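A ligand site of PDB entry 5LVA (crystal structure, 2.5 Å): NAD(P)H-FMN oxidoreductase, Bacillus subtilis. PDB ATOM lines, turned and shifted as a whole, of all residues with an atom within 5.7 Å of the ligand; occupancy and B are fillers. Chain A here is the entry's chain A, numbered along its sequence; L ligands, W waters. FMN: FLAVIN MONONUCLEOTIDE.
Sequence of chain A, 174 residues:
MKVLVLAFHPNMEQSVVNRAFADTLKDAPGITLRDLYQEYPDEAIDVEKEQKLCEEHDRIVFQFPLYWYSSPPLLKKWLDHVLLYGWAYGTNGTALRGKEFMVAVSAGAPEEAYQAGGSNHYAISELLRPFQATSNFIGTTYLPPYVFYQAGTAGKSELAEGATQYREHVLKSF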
ATOM      1  N   HIS A   9      20.655 -15.714  -2.908  1.00  0.00           N
ATOM      2  CA  HIS A   9      20.929 -14.620  -2.022  1.00  0.00           C
ATOM      3  C   HIS A   9      19.884 -14.637  -0.909  1.00  0.00           C
ATOM      4  O   HIS A   9      18.702 -14.702  -1.182  1.00  0.00           O
ATOM      5  CB  HIS A   9      20.922 -13.307  -2.768  1.00  0.00           C
ATOM      6  CG  HIS A   9      21.452 -12.161  -1.977  1.00  0.00           C
ATOM      7  ND1 HIS A   9      20.938 -11.800  -0.753  1.00  0.00           N
ATOM      8  CD2 HIS A   9      22.453 -11.295  -2.235  1.00  0.00           C
ATOM      9  CE1 HIS A   9      21.609 -10.764  -0.283  1.00  0.00           C
ATOM     10  NE2 HIS A   9      22.535 -10.439  -1.166  1.00  0.00           N
ATOM     11  N   GLN A  14      17.208  -6.774   0.078  1.00  0.00           N
ATOM     12  CA  GLN A  14      18.249  -6.005   0.742  1.00  0.00           C
ATOM     13  C   GLN A  14      19.523  -5.989  -0.091  1.00  0.00           C
ATOM     14  O   GLN A  14      20.385  -5.136   0.089  1.00  0.00           O
ATOM     15  CB  GLN A  14      18.525  -6.566   2.139  1.00  0.00           C
ATOM     16  CG  GLN A  14      19.406  -5.699   3.018  1.00  0.00           C
ATOM     17  CD  GLN A  14      19.574  -6.267   4.411  1.00  0.00           C
ATOM     18  OE1 GLN A  14      19.589  -7.478   4.606  1.00  0.00           O
ATOM     19  NE2 GLN A  14      19.705  -5.386   5.393  1.00  0.00           N
ATOM     20  N   SER A  15      19.637  -6.943  -1.007  1.00  0.00           N
ATOM     21  CA  SER A  15      20.769  -7.056  -1.915  1.00  0.00           C
ATOM     22  C   SER A  15      20.966  -5.777  -2.699  1.00  0.00           C
ATOM     23  O   SER A  15      19.996  -5.144  -3.095  1.00  0.00           O
ATOM     24  CB  SER A  15      20.570  -8.224  -2.905  1.00  0.00           C
ATOM     25  OG  SER A  15      21.496  -8.195  -3.967  1.00  0.00           O
ATOM     26  N   VAL A  16      22.213  -5.390  -2.925  1.00  0.00           N
ATOM     27  CA  VAL A  16      22.476  -4.270  -3.810  1.00  0.00           C
ATOM     28  C   VAL A  16      22.940  -4.746  -5.179  1.00  0.00           C
ATOM     29  O   VAL A  16      22.306  -4.422  -6.183  1.00  0.00           O
ATOM     30  CB  VAL A  16      23.530  -3.312  -3.209  1.00  0.00           C
ATOM     31  CG1 VAL A  16      24.037  -2.358  -4.252  1.00  0.00           C
ATOM     32  CG2 VAL A  16      22.919  -2.538  -2.072  1.00  0.00           C
ATOM     33  N   VAL A  17      24.016  -5.528  -5.213  1.00  0.00           N
ATOM     34  CA  VAL A  17      24.657  -5.919  -6.462  1.00  0.00           C
ATOM     35  C   VAL A  17      23.890  -6.971  -7.242  1.00  0.00           C
ATOM     36  O   VAL A  17      23.585  -6.797  -8.418  1.00  0.00           O
ATOM     37  CB  VAL A  17      26.077  -6.450  -6.226  1.00  0.00           C
ATOM     38  CG1 VAL A  17      26.720  -6.871  -7.545  1.00  0.00           C
ATOM     39  CG2 VAL A  17      26.917  -5.423  -5.514  1.00  0.00           C
ATOM     40  N   ASN A  18      23.588  -8.081  -6.587  1.00  0.00           N
ATOM     41  CA  ASN A  18      22.893  -9.166  -7.237  1.00  0.00           C
ATOM     42  C   ASN A  18      21.507  -8.784  -7.681  1.00  0.00           C
ATOM     43  O   ASN A  18      21.038  -9.241  -8.723  1.00  0.00           O
ATOM     44  CB  ASN A  18      22.837 -10.372  -6.316  1.00  0.00           C
ATOM     45  CG  ASN A  18      24.122 -11.168  -6.356  1.00  0.00           C
ATOM     46  OD1 ASN A  18      24.324 -11.979  -7.257  1.00  0.00           O
ATOM     47  ND2 ASN A  18      25.004 -10.917  -5.403  1.00  0.00           N
ATOM     48  N   ARG A  19      20.875  -7.922  -6.902  1.00  0.00           N
ATOM     49  CA  ARG A  19      19.580  -7.360  -7.257  1.00  0.00           C
ATOM     50  C   ARG A  19      19.659  -6.607  -8.591  1.00  0.00           C
ATOM     51  O   ARG A  19      18.839  -6.810  -9.487  1.00  0.00           O
ATOM     52  CB  ARG A  19      19.097  -6.441  -6.137  1.00  0.00           C
ATOM     53  CG  ARG A  19      17.754  -5.807  -6.367  1.00  0.00           C
ATOM     54  CD  ARG A  19      16.723  -6.851  -6.698  1.00  0.00           C
ATOM     55  NE  ARG A  19      15.387  -6.395  -6.346  1.00  0.00           N
ATOM     56  CZ  ARG A  19      14.290  -7.155  -6.415  1.00  0.00           C
ATOM     57  NH1 ARG A  19      14.394  -8.413  -6.834  1.00  0.00           N
ATOM     58  NH2 ARG A  19      13.113  -6.654  -6.073  1.00  0.00           N
ATOM     59  N   PHE A  64      25.320 -15.913  -7.129  1.00  0.00           N
ATOM     60  CA  PHE A  64      25.369 -15.748  -5.687  1.00  0.00           C
ATOM     61  C   PHE A  64      26.443 -14.767  -5.286  1.00  0.00           C
ATOM     62  O   PHE A  64      27.303 -14.458  -6.077  1.00  0.00           O
ATOM     63  CB  PHE A  64      25.601 -17.111  -4.998  1.00  0.00           C
ATOM     64  CG  PHE A  64      26.830 -17.863  -5.496  1.00  0.00           C
ATOM     65  CD1 PHE A  64      26.738 -18.743  -6.555  1.00  0.00           C
ATOM     66  CD2 PHE A  64      28.054 -17.712  -4.857  1.00  0.00           C
ATOM     67  CE1 PHE A  64      27.828 -19.441  -6.983  1.00  0.00           C
ATOM     68  CE2 PHE A  64      29.149 -18.402  -5.281  1.00  0.00           C
ATOM     69  CZ  PHE A  64      29.040 -19.269  -6.345  1.00  0.00           C
ATOM     70  N   PRO A  65      26.350 -14.235  -4.066  1.00  0.00           N
ATOM     71  CA  PRO A  65      27.486 -13.473  -3.561  1.00  0.00           C
ATOM     72  C   PRO A  65      28.542 -14.415  -3.016  1.00  0.00           C
ATOM     73  O   PRO A  65      28.194 -15.476  -2.504  1.00  0.00           O
ATOM     74  CB  PRO A  65      26.874 -12.620  -2.452  1.00  0.00           C
ATOM     75  CG  PRO A  65      25.773 -13.442  -1.949  1.00  0.00           C
ATOM     76  CD  PRO A  65      25.187 -14.111  -3.164  1.00  0.00           C
ATOM     77  N   LEU A  66      29.810 -14.026  -3.118  1.00  0.00           N
ATOM     78  CA  LEU A  66      30.885 -14.774  -2.523  1.00  0.00           C
ATOM     79  C   LEU A  66      30.855 -14.616  -1.018  1.00  0.00           C
ATOM     80  O   LEU A  66      31.134 -13.537  -0.495  1.00  0.00           O
ATOM     81  CB  LEU A  66      32.241 -14.315  -3.059  1.00  0.00           C
ATOM     82  CG  LEU A  66      33.421 -15.254  -2.858  1.00  0.00           C
ATOM     83  CD1 LEU A  66      33.213 -16.488  -3.702  1.00  0.00           C
ATOM     84  CD2 LEU A  66      34.698 -14.561  -3.222  1.00  0.00           C
ATOM     85  N   TYR A  67      30.536 -15.705  -0.330  1.00  0.00           N
ATOM     86  CA  TYR A  67      30.538 -15.767   1.111  1.00  0.00           C
ATOM     87  C   TYR A  67      31.605 -16.730   1.556  1.00  0.00           C
ATOM     88  O   TYR A  67      31.530 -17.904   1.222  1.00  0.00           O
ATOM     89  CB  TYR A  67      29.191 -16.234   1.654  1.00  0.00           C
ATOM     90  CG  TYR A  67      28.062 -15.246   1.600  1.00  0.00           C
ATOM     91  CD1 TYR A  67      28.274 -13.914   1.233  1.00  0.00           C
ATOM     92  CD2 TYR A  67      26.786 -15.627   1.929  1.00  0.00           C
ATOM     93  CE1 TYR A  67      27.235 -13.009   1.205  1.00  0.00           C
ATOM     94  CE2 TYR A  67      25.751 -14.739   1.905  1.00  0.00           C
ATOM     95  CZ  TYR A  67      25.961 -13.435   1.545  1.00  0.00           C
ATOM     96  OH  TYR A  67      24.872 -12.569   1.532  1.00  0.00           O
ATOM     97  N   TRP A  68      32.571 -16.252   2.333  1.00  0.00           N
ATOM     98  CA  TRP A  68      33.749 -17.032   2.757  1.00  0.00           C
ATOM     99  C   TRP A  68      34.288 -17.904   1.627  1.00  0.00           C
ATOM    100  O   TRP A  68      34.513 -19.108   1.771  1.00  0.00           O
ATOM    101  CB  TRP A  68      33.419 -17.855   4.011  1.00  0.00           C
ATOM    102  CG  TRP A  68      33.209 -16.939   5.175  1.00  0.00           C
ATOM    103  CD1 TRP A  68      32.032 -16.632   5.777  1.00  0.00           C
ATOM    104  CD2 TRP A  68      34.211 -16.156   5.834  1.00  0.00           C
ATOM    105  NE1 TRP A  68      32.232 -15.718   6.787  1.00  0.00           N
ATOM    106  CE2 TRP A  68      33.556 -15.403   6.838  1.00  0.00           C
ATOM    107  CE3 TRP A  68      35.590 -16.011   5.668  1.00  0.00           C
ATOM    108  CZ2 TRP A  68      34.243 -14.537   7.681  1.00  0.00           C
ATOM    109  CZ3 TRP A  68      36.272 -15.153   6.508  1.00  0.00           C
ATOM    110  CH2 TRP A  68      35.602 -14.424   7.499  1.00  0.00           C
ATOM    111  N   TYR A  69      34.478 -17.249   0.479  1.00  0.00           N
ATOM    112  CA  TYR A  69      35.099 -17.801  -0.704  1.00  0.00           C
ATOM    113  C   TYR A  69      34.295 -18.967  -1.261  1.00  0.00           C
ATOM    114  O   TYR A  69      34.747 -19.714  -2.118  1.00  0.00           O
ATOM    115  CB  TYR A  69      36.545 -18.210  -0.385  1.00  0.00           C
ATOM    116  CG  TYR A  69      37.273 -17.079   0.311  1.00  0.00           C
ATOM    117  CD1 TYR A  69      37.766 -15.997  -0.402  1.00  0.00           C
ATOM    118  CD2 TYR A  69      37.404 -17.068   1.700  1.00  0.00           C
ATOM    119  CE1 TYR A  69      38.391 -14.957   0.249  1.00  0.00           C
ATOM    120  CE2 TYR A  69      38.029 -16.028   2.350  1.00  0.00           C
ATOM    121  CZ  TYR A  69      38.524 -14.979   1.622  1.00  0.00           C
ATOM    122  OH  TYR A  69      39.144 -13.951   2.277  1.00  0.00           O
ATOM    123  N   SER A  70      33.067 -19.077  -0.787  1.00  0.00           N
ATOM    124  CA  SER A  70      32.134 -20.061  -1.311  1.00  0.00           C
ATOM    125  C   SER A  70      30.775 -19.381  -1.562  1.00  0.00           C
ATOM    126  O   SER A  70      30.712 -18.169  -1.723  1.00  0.00           O
ATOM    127  CB  SER A  70      32.013 -21.237  -0.341  1.00  0.00           C
ATOM    128  OG  SER A  70      31.121 -22.229  -0.824  1.00  0.00           O
ATOM    129  N   SER A 106      29.648 -12.326  -7.109  1.00  0.00           N
ATOM    130  CA  SER A 106      30.084 -10.999  -6.742  1.00  0.00           C
ATOM    131  C   SER A 106      30.968 -11.087  -5.498  1.00  0.00           C
ATOM    132  O   SER A 106      30.708 -11.888  -4.613  1.00  0.00           O
ATOM    133  CB  SER A 106      28.880 -10.092  -6.513  1.00  0.00           C
ATOM    134  OG  SER A 106      28.067 -10.625  -5.487  1.00  0.00           O
ATOM    135  N   ALA A 107      32.009 -10.275  -5.438  1.00  0.00           N
ATOM    136  CA  ALA A 107      32.901 -10.343  -4.296  1.00  0.00           C
ATOM    137  C   ALA A 107      33.191  -8.963  -3.747  1.00  0.00           C
ATOM    138  O   ALA A 107      33.341  -8.018  -4.496  1.00  0.00           O
ATOM    139  CB  ALA A 107      34.197 -11.046  -4.669  1.00  0.00           C
ATOM    140  N   GLY A 108      33.263  -8.857  -2.423  1.00  0.00           N
ATOM    141  CA  GLY A 108      33.523  -7.585  -1.772  1.00  0.00           C
ATOM    142  C   GLY A 108      34.907  -7.029  -2.025  1.00  0.00           C
ATOM    143  O   GLY A 108      35.080  -5.831  -2.226  1.00  0.00           O
ATOM    144  N   ALA A 109      35.902  -7.914  -2.033  1.00  0.00           N
ATOM    145  CA  ALA A 109      37.290  -7.506  -2.147  1.00  0.00           C
ATOM    146  C   ALA A 109      37.652  -7.078  -3.574  1.00  0.00           C
ATOM    147  O   ALA A 109      36.941  -7.399  -4.527  1.00  0.00           O
ATOM    148  CB  ALA A 109      38.183  -8.640  -1.677  1.00  0.00           C
ATOM    149  N   TYR A 114      42.715 -11.142  -5.384  1.00  0.00           N
ATOM    150  CA  TYR A 114      42.570 -12.526  -5.800  1.00  0.00           C
ATOM    151  C   TYR A 114      43.653 -12.966  -6.791  1.00  0.00           C
ATOM    152  O   TYR A 114      43.406 -13.151  -7.965  1.00  0.00           O
ATOM    153  CB  TYR A 114      41.168 -12.765  -6.371  1.00  0.00           C
ATOM    154  CG  TYR A 114      40.120 -12.637  -5.288  1.00  0.00           C
ATOM    155  CD1 TYR A 114      39.944 -13.649  -4.372  1.00  0.00           C
ATOM    156  CD2 TYR A 114      39.351 -11.507  -5.158  1.00  0.00           C
ATOM    157  CE1 TYR A 114      39.023 -13.549  -3.369  1.00  0.00           C
ATOM    158  CE2 TYR A 114      38.409 -11.386  -4.145  1.00  0.00           C
ATOM    159  CZ  TYR A 114      38.258 -12.422  -3.263  1.00  0.00           C
ATOM    160  OH  TYR A 114      37.337 -12.331  -2.242  1.00  0.00           O
ATOM    161  N   ASN A 120      44.308 -11.870  -0.783  1.00  0.00           N
ATOM    162  CA  ASN A 120      43.594 -13.132  -0.640  1.00  0.00           C
ATOM    163  C   ASN A 120      44.328 -14.311  -1.274  1.00  0.00           C
ATOM    164  O   ASN A 120      43.893 -15.456  -1.127  1.00  0.00           O
ATOM    165  CB  ASN A 120      42.191 -13.006  -1.221  1.00  0.00           C
ATOM    166  CG  ASN A 120      41.250 -12.319  -0.263  1.00  0.00           C
ATOM    167  OD1 ASN A 120      41.437 -12.362   0.955  1.00  0.00           O
ATOM    168  ND2 ASN A 120      40.224 -11.682  -0.802  1.00  0.00           N
ATOM    169  N   ALA A 151      32.278  -5.321  -4.843  1.00  0.00           N
ATOM    170  CA  ALA A 151      30.837  -5.340  -4.771  1.00  0.00           C
ATOM    171  C   ALA A 151      30.311  -4.607  -3.532  1.00  0.00           C
ATOM    172  O   ALA A 151      30.698  -4.910  -2.408  1.00  0.00           O
ATOM    173  CB  ALA A 151      30.339  -6.774  -4.790  1.00  0.00           C
ATOM    174  N   GLY A 152      29.447  -3.626  -3.755  1.00  0.00           N
ATOM    175  CA  GLY A 152      28.945  -2.790  -2.676  1.00  0.00           C
ATOM    176  C   GLY A 152      29.607  -1.438  -2.519  1.00  0.00           C
ATOM    177  O   GLY A 152      28.983  -0.491  -2.077  1.00  0.00           O
HETATM  178  N1  FMN L   1      33.690 -10.832  -0.184  1.00  0.00           N
HETATM  179  C2  FMN L   1      34.854 -11.380  -0.671  1.00  0.00           C
HETATM  180  O2  FMN L   1      35.497 -10.803  -1.543  1.00  0.00           O
HETATM  181  N3  FMN L   1      35.303 -12.590  -0.206  1.00  0.00           N
HETATM  182  C4  FMN L   1      34.607 -13.266   0.750  1.00  0.00           C
HETATM  183  O4  FMN L   1      35.049 -14.342   1.136  1.00  0.00           O
HETATM  184  C4A FMN L   1      33.431 -12.709   1.264  1.00  0.00           C
HETATM  185  N5  FMN L   1      32.714 -13.363   2.231  1.00  0.00           N
HETATM  186  C5A FMN L   1      31.555 -12.836   2.730  1.00  0.00           C
HETATM  187  C6  FMN L   1      30.858 -13.525   3.713  1.00  0.00           C
HETATM  188  C7  FMN L   1      29.675 -13.030   4.230  1.00  0.00           C
HETATM  189  C7M FMN L   1      28.940 -13.805   5.282  1.00  0.00           C
HETATM  190  C8  FMN L   1      29.199 -11.802   3.762  1.00  0.00           C
HETATM  191  C8M FMN L   1      27.926 -11.217   4.289  1.00  0.00           C
HETATM  192  C9  FMN L   1      29.909 -11.110   2.781  1.00  0.00           C
HETATM  193  C9A FMN L   1      31.082 -11.620   2.256  1.00  0.00           C
HETATM  194  N10 FMN L   1      31.801 -10.937   1.281  1.00  0.00           N
HETATM  195  C10 FMN L   1      32.973 -11.490   0.792  1.00  0.00           C
HETATM  196  C1' FMN L   1      31.282  -9.638   0.726  1.00  0.00           C
HETATM  197  C2' FMN L   1      30.284 -10.095  -0.363  1.00  0.00           C
HETATM  198  O2' FMN L   1      30.919 -10.888  -1.364  1.00  0.00           O
HETATM  199  C3' FMN L   1      29.410  -8.984  -0.990  1.00  0.00           C
HETATM  200  O3' FMN L   1      28.612  -8.512   0.063  1.00  0.00           O
HETATM  201  C4' FMN L   1      28.540  -9.552  -2.123  1.00  0.00           C
HETATM  202  O4' FMN L   1      29.369 -10.147  -3.070  1.00  0.00           O
HETATM  203  C5' FMN L   1      27.670  -8.621  -2.962  1.00  0.00           C
HETATM  204  O5' FMN L   1      26.525  -8.246  -2.226  1.00  0.00           O
HETATM  205  P   FMN L   1      25.003  -8.141  -2.740  1.00  0.00           P
HETATM  206  O1P FMN L   1      24.263  -8.760  -1.610  1.00  0.00           O
HETATM  207  O2P FMN L   1      24.673  -6.694  -2.931  1.00  0.00           O
HETATM  208  O3P FMN L   1      24.628  -8.886  -3.968  1.00  0.00           O
HETATM  209  O   HOH W   1      29.012  -5.856  -0.286  1.00  0.00           O
HETATM  210  O   HOH W   2      26.630  -4.933  -1.505  1.00  0.00           O
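O of Phe 64 is in hydrogen-bond range of N of Ser 106.
The side-chain hydroxyl (OH) of Tyr 114 sits close to the side-chain amide nitrogen (ND2) of Asn 120 (3.3 Å).
The side-chain amide oxygen (OD1) of Asn 120 sits at hydrogen-bond distance from the side-chain hydroxyl (OH) of Tyr 69 (3.1 Å).
The backbone NH (N) of Asn 18 is in hydrogen-bond range of the side-chain hydroxyl (OG) of Ser 15 (3.4 Å).
N of Arg 19 sits at hydrogen-bond distance from OG of Ser 15, 3.0 Å away.
The backbone carbonyl oxygen of Ala 107 is in hydrogen-bond range of the backbone NH of Ala 151 (2.9 Å).
O of Ser 106 sits at hydrogen-bond distance from N of Leu 66 (2.8 Å).
The side-chain amide nitrogen (ND2) of Asn 18 is in hydrogen-bond range of the side-chain hydroxyl (OG) of Ser 106, 3.1 Å away.
Merely in contact with the ligand: Ala 107, Tyr 67, Pro 65 and Ala 151.
16 residues have an atom within 4 Å of the ligand: His 9, Ser 15, Val 16, Val 17, Asn 18, Pro 65, Leu 66, Tyr 67, Trp 68, Tyr 69, Ser 106, Ala 107, Gly 108, Ala 109, Tyr 114 and Ala 151.
The nearest printed residue that does not touch the ligand is Arg 19 (4.9 Å).
OG of Ser 106 sits at hydrogen-bond distance from O4' of the ligand (2.8 Å).
O of Leu 66 lies within hydrogen-bond range of O2' of the ligand (2.8 Å).
The side-chain hydroxyl (OG) of Ser 15 lies within hydrogen-bond range of an oxygen (O3P) of the ligand (3.2 Å).
The backbone NH (N) of Gly 108 lies within hydrogen-bond range of a nitrogen (N1) of the ligand (3.0 Å).
The backbone NH (N) of Val 17 is in hydrogen-bond range of an oxygen (O2P) of the ligand (2.6 Å).
The backbone NH (N) of Trp 68 is in hydrogen-bond range of a nitrogen (N5) of the ligand (2.9 Å).
The backbone NH (N) of Tyr 69 is in hydrogen-bond range of an oxygen (O4) of the ligand, 3.0 Å away.
N of Asn 18 sits at hydrogen-bond distance from O3P of the ligand (2.9 Å).
An oxygen (O3P) of the ligand lies within hydrogen-bond range of the side-chain amide nitrogen of Asn 18 (2.5 Å).
An oxygen (O2) of the ligand is in hydrogen-bond range of the side-chain hydroxyl (OH) of Tyr 114 (2.5 Å).
The backbone carbonyl oxygen (O) of Ser 106 sits at hydrogen-bond distance from an oxygen (O4') of the ligand.
The backbone NH (N) of Val 16 sits at hydrogen-bond distance from an oxygen (O2P) of the ligand (2.8 Å).
A ring nitrogen (NE2) of His 9 is in hydrogen-bond range of an oxygen (O1P) of the ligand (2.4 Å).
The backbone NH of Ala 109 is in hydrogen-bond range of an oxygen (O2) of the ligand (3.0 Å).
Water W1 lies within hydrogen-bond range of O3' of the ligand (2.7 Å) and O of Ala 151 (2.9 Å).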
